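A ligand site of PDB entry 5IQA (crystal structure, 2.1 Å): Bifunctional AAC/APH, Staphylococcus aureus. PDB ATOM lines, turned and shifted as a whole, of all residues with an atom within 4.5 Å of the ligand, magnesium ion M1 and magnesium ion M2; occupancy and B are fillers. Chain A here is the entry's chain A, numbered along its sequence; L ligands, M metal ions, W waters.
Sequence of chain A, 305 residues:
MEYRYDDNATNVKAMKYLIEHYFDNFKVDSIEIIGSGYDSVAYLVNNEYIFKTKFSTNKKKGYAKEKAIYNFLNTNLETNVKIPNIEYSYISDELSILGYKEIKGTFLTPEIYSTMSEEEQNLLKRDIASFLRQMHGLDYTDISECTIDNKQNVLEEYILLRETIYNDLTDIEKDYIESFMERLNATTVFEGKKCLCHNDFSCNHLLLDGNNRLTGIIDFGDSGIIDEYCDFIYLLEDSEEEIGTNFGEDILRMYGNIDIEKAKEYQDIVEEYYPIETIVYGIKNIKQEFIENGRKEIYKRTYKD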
ATOM      1  N   ILE A  34     -23.444   3.037 -20.793  1.00  0.00           N
ATOM      2  CA  ILE A  34     -23.897   4.384 -20.426  1.00  0.00           C
ATOM      3  C   ILE A  34     -25.285   4.683 -20.987  1.00  0.00           C
ATOM      4  O   ILE A  34     -25.956   5.566 -20.525  1.00  0.00           O
ATOM      5  CB  ILE A  34     -22.851   5.414 -20.885  1.00  0.00           C
ATOM      6  CG1 ILE A  34     -23.008   6.729 -20.115  1.00  0.00           C
ATOM      7  CG2 ILE A  34     -22.883   5.633 -22.394  1.00  0.00           C
ATOM      8  CD1 ILE A  34     -22.548   6.643 -18.665  1.00  0.00           C
ATOM      9  N   GLY A  35     -25.716   3.955 -22.004  1.00  0.00           N
ATOM     10  CA  GLY A  35     -27.076   4.079 -22.536  1.00  0.00           C
ATOM     11  C   GLY A  35     -27.497   2.973 -23.513  1.00  0.00           C
ATOM     12  O   GLY A  35     -26.667   2.172 -23.958  1.00  0.00           O
ATOM     13  N   SER A  36     -28.793   2.942 -23.799  1.00  0.00           N
ATOM     14  CA  SER A  36     -29.440   1.883 -24.592  1.00  0.00           C
ATOM     15  C   SER A  36     -30.665   2.360 -25.285  1.00  0.00           C
ATOM     16  O   SER A  36     -31.493   3.040 -24.702  1.00  0.00           O
ATOM     17  CB  SER A  36     -29.968   0.768 -23.713  1.00  0.00           C
ATOM     18  OG  SER A  36     -28.884   0.115 -23.151  1.00  0.00           O
ATOM     19  N   GLY A  37     -30.773   1.983 -26.544  1.00  0.00           N
ATOM     20  CA  GLY A  37     -32.007   2.126 -27.301  1.00  0.00           C
ATOM     21  C   GLY A  37     -32.528   0.718 -27.487  1.00  0.00           C
ATOM     22  O   GLY A  37     -32.122  -0.218 -26.771  1.00  0.00           O
ATOM     23  N   SER A  40     -29.640  -0.609 -30.032  1.00  0.00           N
ATOM     24  CA  SER A  40     -28.306  -0.124 -29.921  1.00  0.00           C
ATOM     25  C   SER A  40     -27.849  -0.063 -28.480  1.00  0.00           C
ATOM     26  O   SER A  40     -28.668   0.023 -27.567  1.00  0.00           O
ATOM     27  CB  SER A  40     -28.192   1.280 -30.519  1.00  0.00           C
ATOM     28  OG  SER A  40     -28.815   2.219 -29.638  1.00  0.00           O
ATOM     29  N   ALA A  42     -24.767   2.063 -26.060  1.00  0.00           N
ATOM     30  CA  ALA A  42     -23.646   2.985 -25.923  1.00  0.00           C
ATOM     31  C   ALA A  42     -22.799   2.665 -24.731  1.00  0.00           C
ATOM     32  O   ALA A  42     -23.297   2.438 -23.656  1.00  0.00           O
ATOM     33  CB  ALA A  42     -24.158   4.410 -25.857  1.00  0.00           C
ATOM     34  N   ILE A  50     -16.886   7.756 -25.867  1.00  0.00           N
ATOM     35  CA  ILE A  50     -18.195   7.119 -26.067  1.00  0.00           C
ATOM     36  C   ILE A  50     -18.064   6.245 -27.297  1.00  0.00           C
ATOM     37  O   ILE A  50     -17.553   6.692 -28.335  1.00  0.00           O
ATOM     38  CB  ILE A  50     -19.285   8.146 -26.385  1.00  0.00           C
ATOM     39  CG1 ILE A  50     -19.470   9.122 -25.217  1.00  0.00           C
ATOM     40  CG2 ILE A  50     -20.596   7.470 -26.743  1.00  0.00           C
ATOM     41  CD1 ILE A  50     -20.148   8.542 -23.988  1.00  0.00           C
ATOM     42  N   LYS A  52     -20.732   4.144 -29.553  1.00  0.00           N
ATOM     43  CA  LYS A  52     -22.077   3.749 -29.930  1.00  0.00           C
ATOM     44  C   LYS A  52     -22.008   2.536 -30.813  1.00  0.00           C
ATOM     45  O   LYS A  52     -21.255   2.546 -31.761  1.00  0.00           O
ATOM     46  CB  LYS A  52     -22.783   4.832 -30.750  1.00  0.00           C
ATOM     47  CG  LYS A  52     -23.280   6.054 -29.989  1.00  0.00           C
ATOM     48  CD  LYS A  52     -23.962   7.083 -30.886  1.00  0.00           C
ATOM     49  CE  LYS A  52     -25.396   6.711 -31.189  1.00  0.00           C
ATOM     50  NZ  LYS A  52     -26.125   7.942 -31.688  1.00  0.00           N
ATOM     51  N   TYR A  63     -25.380   3.854 -39.064  1.00  0.00           N
ATOM     52  CA  TYR A  63     -24.247   4.615 -38.542  1.00  0.00           C
ATOM     53  C   TYR A  63     -23.410   5.260 -39.648  1.00  0.00           C
ATOM     54  O   TYR A  63     -22.771   6.265 -39.377  1.00  0.00           O
ATOM     55  CB  TYR A  63     -23.452   3.928 -37.506  1.00  0.00           C
ATOM     56  CG  TYR A  63     -24.146   3.785 -36.157  1.00  0.00           C
ATOM     57  CD1 TYR A  63     -25.475   4.205 -35.967  1.00  0.00           C
ATOM     58  CD2 TYR A  63     -23.502   3.150 -35.076  1.00  0.00           C
ATOM     59  CE1 TYR A  63     -26.086   4.050 -34.751  1.00  0.00           C
ATOM     60  CE2 TYR A  63     -24.151   2.961 -33.842  1.00  0.00           C
ATOM     61  CZ  TYR A  63     -25.407   3.424 -33.688  1.00  0.00           C
ATOM     62  OH  TYR A  63     -26.061   3.310 -32.496  1.00  0.00           O
ATOM     63  N   GLU A  66     -24.958   8.796 -39.889  1.00  0.00           N
ATOM     64  CA  GLU A  66     -24.680   9.578 -38.697  1.00  0.00           C
ATOM     65  C   GLU A  66     -23.237  10.070 -38.762  1.00  0.00           C
ATOM     66  O   GLU A  66     -22.946  11.249 -38.526  1.00  0.00           O
ATOM     67  CB  GLU A  66     -24.933   8.725 -37.451  1.00  0.00           C
ATOM     68  CG  GLU A  66     -24.637   9.435 -36.164  1.00  0.00           C
ATOM     69  CD  GLU A  66     -25.238   8.755 -34.953  1.00  0.00           C
ATOM     70  OE1 GLU A  66     -26.025   7.747 -35.113  1.00  0.00           O
ATOM     71  OE2 GLU A  66     -24.964   9.297 -33.833  1.00  0.00           O
ATOM     72  N   TYR A 100     -16.028   8.401 -30.191  1.00  0.00           N
ATOM     73  CA  TYR A 100     -15.642   9.812 -30.106  1.00  0.00           C
ATOM     74  C   TYR A 100     -15.413  10.186 -28.670  1.00  0.00           C
ATOM     75  O   TYR A 100     -15.883   9.484 -27.765  1.00  0.00           O
ATOM     76  CB  TYR A 100     -16.739  10.692 -30.731  1.00  0.00           C
ATOM     77  CG  TYR A 100     -18.120  10.513 -30.150  1.00  0.00           C
ATOM     78  CD1 TYR A 100     -18.533  11.254 -29.070  1.00  0.00           C
ATOM     79  CD2 TYR A 100     -19.025   9.625 -30.701  1.00  0.00           C
ATOM     80  CE1 TYR A 100     -19.803  11.095 -28.540  1.00  0.00           C
ATOM     81  CE2 TYR A 100     -20.303   9.480 -30.187  1.00  0.00           C
ATOM     82  CZ  TYR A 100     -20.677  10.189 -29.086  1.00  0.00           C
ATOM     83  OH  TYR A 100     -21.973  10.074 -28.594  1.00  0.00           O
ATOM     84  N   GLU A 102     -15.963  11.786 -25.275  1.00  0.00           N
ATOM     85  CA  GLU A 102     -17.109  12.115 -24.516  1.00  0.00           C
ATOM     86  C   GLU A 102     -17.173  13.624 -24.326  1.00  0.00           C
ATOM     87  O   GLU A 102     -16.230  14.247 -23.807  1.00  0.00           O
ATOM     88  CB  GLU A 102     -17.051  11.486 -23.129  1.00  0.00           C
ATOM     89  CG  GLU A 102     -18.253  11.817 -22.235  1.00  0.00           C
ATOM     90  CD  GLU A 102     -18.040  11.470 -20.763  1.00  0.00           C
ATOM     91  OE1 GLU A 102     -16.888  11.444 -20.300  1.00  0.00           O
ATOM     92  OE2 GLU A 102     -19.043  11.261 -20.026  1.00  0.00           O
ATOM     93  N   ILE A 103     -18.330  14.192 -24.596  1.00  0.00           N
ATOM     94  CA  ILE A 103     -18.535  15.611 -24.225  1.00  0.00           C
ATOM     95  C   ILE A 103     -18.962  15.685 -22.794  1.00  0.00           C
ATOM     96  O   ILE A 103     -19.898  15.020 -22.402  1.00  0.00           O
ATOM     97  CB  ILE A 103     -19.571  16.277 -25.113  1.00  0.00           C
ATOM     98  CG1 ILE A 103     -19.090  16.219 -26.567  1.00  0.00           C
ATOM     99  CG2 ILE A 103     -19.789  17.732 -24.692  1.00  0.00           C
ATOM    100  CD1 ILE A 103     -20.225  16.337 -27.539  1.00  0.00           C
ATOM    101  N   PHE A 107     -26.796  16.566 -18.286  1.00  0.00           N
ATOM    102  CA  PHE A 107     -27.923  16.608 -19.161  1.00  0.00           C
ATOM    103  C   PHE A 107     -29.010  17.484 -18.575  1.00  0.00           C
ATOM    104  O   PHE A 107     -29.287  17.411 -17.432  1.00  0.00           O
ATOM    105  CB  PHE A 107     -28.459  15.196 -19.551  1.00  0.00           C
ATOM    106  CG  PHE A 107     -27.595  14.511 -20.582  1.00  0.00           C
ATOM    107  CD1 PHE A 107     -27.547  14.983 -21.867  1.00  0.00           C
ATOM    108  CD2 PHE A 107     -26.689  13.501 -20.180  1.00  0.00           C
ATOM    109  CE1 PHE A 107     -26.693  14.412 -22.804  1.00  0.00           C
ATOM    110  CE2 PHE A 107     -25.814  12.945 -21.103  1.00  0.00           C
ATOM    111  CZ  PHE A 107     -25.827  13.413 -22.415  1.00  0.00           C
ATOM    112  N   ASP A 200     -33.932  15.083 -33.421  1.00  0.00           N
ATOM    113  CA  ASP A 200     -34.317  14.338 -32.188  1.00  0.00           C
ATOM    114  C   ASP A 200     -33.979  15.201 -30.982  1.00  0.00           C
ATOM    115  O   ASP A 200     -33.303  14.774 -30.036  1.00  0.00           O
ATOM    116  CB  ASP A 200     -33.588  13.002 -32.167  1.00  0.00           C
ATOM    117  CG  ASP A 200     -34.197  11.970 -31.220  1.00  0.00           C
ATOM    118  OD1 ASP A 200     -35.294  12.171 -30.639  1.00  0.00           O
ATOM    119  OD2 ASP A 200     -33.588  10.892 -31.114  1.00  0.00           O
ATOM    120  N   ASN A 204     -32.820  15.343 -23.165  1.00  0.00           N
ATOM    121  CA  ASN A 204     -31.804  14.314 -22.884  1.00  0.00           C
ATOM    122  C   ASN A 204     -30.634  14.245 -23.908  1.00  0.00           C
ATOM    123  O   ASN A 204     -29.735  13.390 -23.790  1.00  0.00           O
ATOM    124  CB  ASN A 204     -32.467  12.932 -22.709  1.00  0.00           C
ATOM    125  CG  ASN A 204     -33.011  12.383 -24.001  1.00  0.00           C
ATOM    126  OD1 ASN A 204     -33.589  13.100 -24.773  1.00  0.00           O
ATOM    127  ND2 ASN A 204     -32.708  11.157 -24.298  1.00  0.00           N
ATOM    128  N   HIS A 205     -30.637  15.118 -24.913  1.00  0.00           N
ATOM    129  CA  HIS A 205     -29.512  15.246 -25.768  1.00  0.00           C
ATOM    130  C   HIS A 205     -28.764  16.568 -25.597  1.00  0.00           C
ATOM    131  O   HIS A 205     -27.830  16.845 -26.379  1.00  0.00           O
ATOM    132  CB  HIS A 205     -29.914  15.070 -27.209  1.00  0.00           C
ATOM    133  CG  HIS A 205     -30.382  13.689 -27.540  1.00  0.00           C
ATOM    134  ND1 HIS A 205     -31.341  13.441 -28.491  1.00  0.00           N
ATOM    135  CD2 HIS A 205     -29.996  12.467 -27.082  1.00  0.00           C
ATOM    136  CE1 HIS A 205     -31.562  12.141 -28.583  1.00  0.00           C
ATOM    137  NE2 HIS A 205     -30.733  11.515 -27.761  1.00  0.00           N
ATOM    138  N   LEU A 207     -26.447  19.083 -23.238  1.00  0.00           N
ATOM    139  CA  LEU A 207     -25.492  19.071 -22.077  1.00  0.00           C
ATOM    140  C   LEU A 207     -25.252  20.488 -21.590  1.00  0.00           C
ATOM    141  O   LEU A 207     -24.994  21.412 -22.387  1.00  0.00           O
ATOM    142  CB  LEU A 207     -24.164  18.482 -22.489  1.00  0.00           C
ATOM    143  CG  LEU A 207     -24.167  16.953 -22.621  1.00  0.00           C
ATOM    144  CD1 LEU A 207     -23.072  16.442 -23.516  1.00  0.00           C
ATOM    145  CD2 LEU A 207     -24.026  16.285 -21.224  1.00  0.00           C
ATOM    146  N   ILE A 218     -25.622  16.057 -28.402  1.00  0.00           N
ATOM    147  CA  ILE A 218     -25.309  14.714 -28.889  1.00  0.00           C
ATOM    148  C   ILE A 218     -26.426  14.137 -29.741  1.00  0.00           C
ATOM    149  O   ILE A 218     -27.513  14.702 -29.862  1.00  0.00           O
ATOM    150  CB  ILE A 218     -25.017  13.756 -27.729  1.00  0.00           C
ATOM    151  CG1 ILE A 218     -26.232  13.649 -26.801  1.00  0.00           C
ATOM    152  CG2 ILE A 218     -23.811  14.254 -26.949  1.00  0.00           C
ATOM    153  CD1 ILE A 218     -26.161  12.360 -25.983  1.00  0.00           C
ATOM    154  N   ASP A 219     -26.107  13.007 -30.320  1.00  0.00           N
ATOM    155  CA  ASP A 219     -27.087  12.140 -31.059  1.00  0.00           C
ATOM    156  C   ASP A 219     -27.739  12.839 -32.210  1.00  0.00           C
ATOM    157  O   ASP A 219     -28.921  13.155 -32.162  1.00  0.00           O
ATOM    158  CB  ASP A 219     -28.140  11.547 -30.132  1.00  0.00           C
ATOM    159  CG  ASP A 219     -28.891  10.387 -30.787  1.00  0.00           C
ATOM    160  OD1 ASP A 219     -28.642  10.106 -31.962  1.00  0.00           O
ATOM    161  OD2 ASP A 219     -29.753   9.755 -30.131  1.00  0.00           O
ATOM    162  N   GLY A 221     -28.082  11.233 -34.866  1.00  0.00           N
ATOM    163  CA  GLY A 221     -28.355  10.048 -35.624  1.00  0.00           C
ATOM    164  C   GLY A 221     -29.564  10.175 -36.573  1.00  0.00           C
ATOM    165  O   GLY A 221     -29.615   9.504 -37.602  1.00  0.00           O
HETATM  166  P1  LIG L   1     -29.350   5.691 -31.546  1.00  0.00           P
HETATM  167  O1  LIG L   1     -30.791   5.447 -31.631  1.00  0.00           O
HETATM  168  O2  LIG L   1     -28.483   4.693 -32.509  1.00  0.00           O
HETATM  169  O3  LIG L   1     -28.808   7.224 -31.667  1.00  0.00           O
HETATM  170  N1  LIG L   1     -28.920   5.372 -29.994  1.00  0.00           N
HETATM  171  P2  LIG L   1     -28.986   6.334 -28.677  1.00  0.00           P
HETATM  172  O4  LIG L   1     -30.111   7.265 -28.744  1.00  0.00           O
HETATM  173  O5  LIG L   1     -29.110   5.388 -27.402  1.00  0.00           O
HETATM  174  O6  LIG L   1     -27.628   7.095 -28.578  1.00  0.00           O
HETATM  175  P3  LIG L   1     -27.137   8.479 -27.965  1.00  0.00           P
HETATM  176  O7  LIG L   1     -28.335   9.247 -27.553  1.00  0.00           O
HETATM  177  O8  LIG L   1     -26.219   9.117 -28.977  1.00  0.00           O
HETATM  178  O9  LIG L   1     -26.223   8.104 -26.723  1.00  0.00           O
HETATM  179  C1  LIG L   1     -26.771   7.243 -25.711  1.00  0.00           C
HETATM  180  C2  LIG L   1     -26.502   7.844 -24.343  1.00  0.00           C
HETATM  181  O10 LIG L   1     -25.082   7.903 -24.134  1.00  0.00           O
HETATM  182  C3  LIG L   1     -26.974   9.268 -24.117  1.00  0.00           C
HETATM  183  O11 LIG L   1     -28.263   9.290 -23.521  1.00  0.00           O
HETATM  184  C4  LIG L   1     -26.056   9.717 -23.020  1.00  0.00           C
HETATM  185  O12 LIG L   1     -26.298   9.027 -21.790  1.00  0.00           O
HETATM  186  C5  LIG L   1     -24.741   9.076 -23.431  1.00  0.00           C
HETATM  187  N2  LIG L   1     -23.855   9.906 -24.271  1.00  0.00           N
HETATM  188  C6  LIG L   1     -23.572   9.755 -25.603  1.00  0.00           C
HETATM  189  N3  LIG L   1     -22.685  10.637 -26.040  1.00  0.00           N
HETATM  190  C7  LIG L   1     -22.382  11.390 -24.925  1.00  0.00           C
HETATM  191  C8  LIG L   1     -21.460  12.440 -24.729  1.00  0.00           C
HETATM  192  O13 LIG L   1     -20.761  12.920 -25.579  1.00  0.00           O
HETATM  193  N4  LIG L   1     -21.390  12.885 -23.430  1.00  0.00           N
HETATM  194  C9  LIG L   1     -22.119  12.348 -22.390  1.00  0.00           C
HETATM  195  N5  LIG L   1     -22.004  12.925 -21.195  1.00  0.00           N
HETATM  196  N6  LIG L   1     -22.982  11.341 -22.545  1.00  0.00           N
HETATM  197  C10 LIG L   1     -23.084  10.936 -23.824  1.00  0.00           C
HETATM  198 MG    MG M   1     -30.337   9.333 -28.126  1.00  0.00          MG
HETATM  199 MG    MG M   2     -30.243   8.584 -32.034  1.00  0.00          MG
HETATM  200  O   HOH W   1     -20.052  13.903 -18.849  1.00  0.00           O
HETATM  201  O   HOH W   2     -31.979   7.636 -31.401  1.00  0.00           O
HETATM  202  O   HOH W   3     -28.479   7.174 -21.466  1.00  0.00           O
HETATM  203  O   HOH W   4     -29.356  11.597 -21.627  1.00  0.00           O
HETATM  204  O   HOH W   5     -30.968   8.968 -26.371  1.00  0.00           O
HETATM  205  O   HOH W   6     -30.514   6.276 -25.345  1.00  0.00           O
HETATM  206  O   HOH W   7     -24.347  10.826 -29.716  1.00  0.00           O
HETATM  207  O   HOH W   8     -31.558  10.344 -32.635  1.00  0.00           O
HETATM  208  O   HOH W   9     -31.323   9.322 -22.077  1.00  0.00           O
HETATM  209  O   HOH W  10     -30.073   2.962 -33.495  1.00  0.00           O
HETATM  210  O   HOH W  11     -32.258   8.995 -28.895  1.00  0.00           O
HETATM  211  O   HOH W  12     -30.162   8.279 -34.123  1.00  0.00           O
HETATM  212  O   HOH W  13     -27.674   3.033 -27.635  1.00  0.00           O
HETATM  213  O   HOH W  14     -28.458   6.352 -35.117  1.00  0.00           O
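Ile 34 touches the ligand (CG2 to O10, 3.6 Å).
Gly 37 touches the ligand.
Ala 42 touches the ligand.
Ile 50 touches the ligand.
Glu 102 touches the ligand (CG to N4, 3.5 Å).
CZ of Phe 107 touches N6 of the ligand, 3.5 Å away.
CD2 of Leu 207 touches N5 of the ligand, 3.9 Å away.
CG2 of Ile 218 touches O13 of the ligand (3.6 Å).
Hydrophobic or aromatic side chains that line the ligand: Ile 34, Ala 42, Ile 50, Tyr 63, Tyr 100, Ile 103, Phe 107, His 205, Leu 207 and Ile 218.
Of the 21 residues printed, 15 come within 4 Å of the ligand.
The nearest printed residue that does not touch magnesium ion M1 is Asp 200 (4.7 Å).
O3 of the ligand is bound to magnesium ion M2 (2.0 Å).
Water W2 is bound to magnesium ion M2, at 2.1 Å.
Magnesium ion M2 is bound by water W12 (2.1 Å).
Magnesium ion M2 is bound by the side-chain carboxylate (OD1) of Asp 219.
Magnesium ion M2 is bound by water W8, at 2.3 Å.
Magnesium ion M2 is bound by the side-chain carboxylate (OD2) of Asp 219 (2.3 Å).
Magnesium ion M2 has six donor atoms within binding distance.
Magnesium ion M1 is bound by water W5 (1.9 Å), O7 of the ligand (2.1 Å), water W11 (2.1 Å), OD2 of Asp 219 (2.1 Å), O4 of the ligand (2.2 Å) and NE2 of His 205 (2.2 Å).
Water W7 lies within hydrogen-bond range of an oxygen (O8) of the ligand (2.6 Å), the side-chain hydroxyl (OH) of Tyr 100 (2.7 Å) and the backbone NH (N) of Asp 219 (2.9 Å).
Water W6 bridges an oxygen (O5) of the ligand and the backbone carbonyl oxygen of Ser 36.
Water W14 lies within hydrogen-bond range of OE1 of Glu 66 (2.8 Å) and O2 of the ligand (3.1 Å).
Water W4 bridges O of Asn 204 (2.8 Å) and O11 of the ligand (3.2 Å).
Water W1 bridges OE2 of Glu 102 (3.1 Å) and N5 of the ligand (3.2 Å).
Water W9 bridges ND2 of Asn 204 and O11 of the ligand.
OH of Tyr 63 sits at hydrogen-bond distance from O2 of the ligand (2.8 Å).
An oxygen (O8) of the ligand is in salt-bridge range of the side-chain amino group (NZ) of Lys 52.
The backbone carbonyl oxygen (O) of Ile 103 sits at hydrogen-bond distance from a nitrogen (N4) of the ligand.
An oxygen (O13) of the ligand is in hydrogen-bond range of the backbone NH of Ile 103 (2.9 Å).
A nitrogen (N1) of the ligand is in hydrogen-bond range of the side-chain hydroxyl (OG) of Ser 40 (3.2 Å).
OH of Tyr 100 is in hydrogen-bond range of N3 of the ligand (2.7 Å).
The backbone carbonyl oxygen of Ala 42 is in hydrogen-bond range of the backbone NH of Ile 34.
O of Gly 35 sits at hydrogen-bond distance from N of Ala 42, at 2.8 Å.
The backbone carbonyl oxygen of Tyr 100 is in hydrogen-bond range of the backbone NH of Ile 50 (2.8 Å).
The side-chain amino group (NZ) of Lys 52 sits close to the side-chain carboxylate (OD1) of Asp 219.
O of Asp 200 sits at hydrogen-bond distance from ND1 of His 205.
N of Gly 221 lies close to OD1 of Asp 219.
The side-chain amino group (NZ) of Lys 52 is in salt-bridge range of the side-chain carboxylate (OE2) of Glu 66 (2.8 Å).
The backbone NH of Ile 218 is in hydrogen-bond range of the backbone carbonyl oxygen of His 205.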
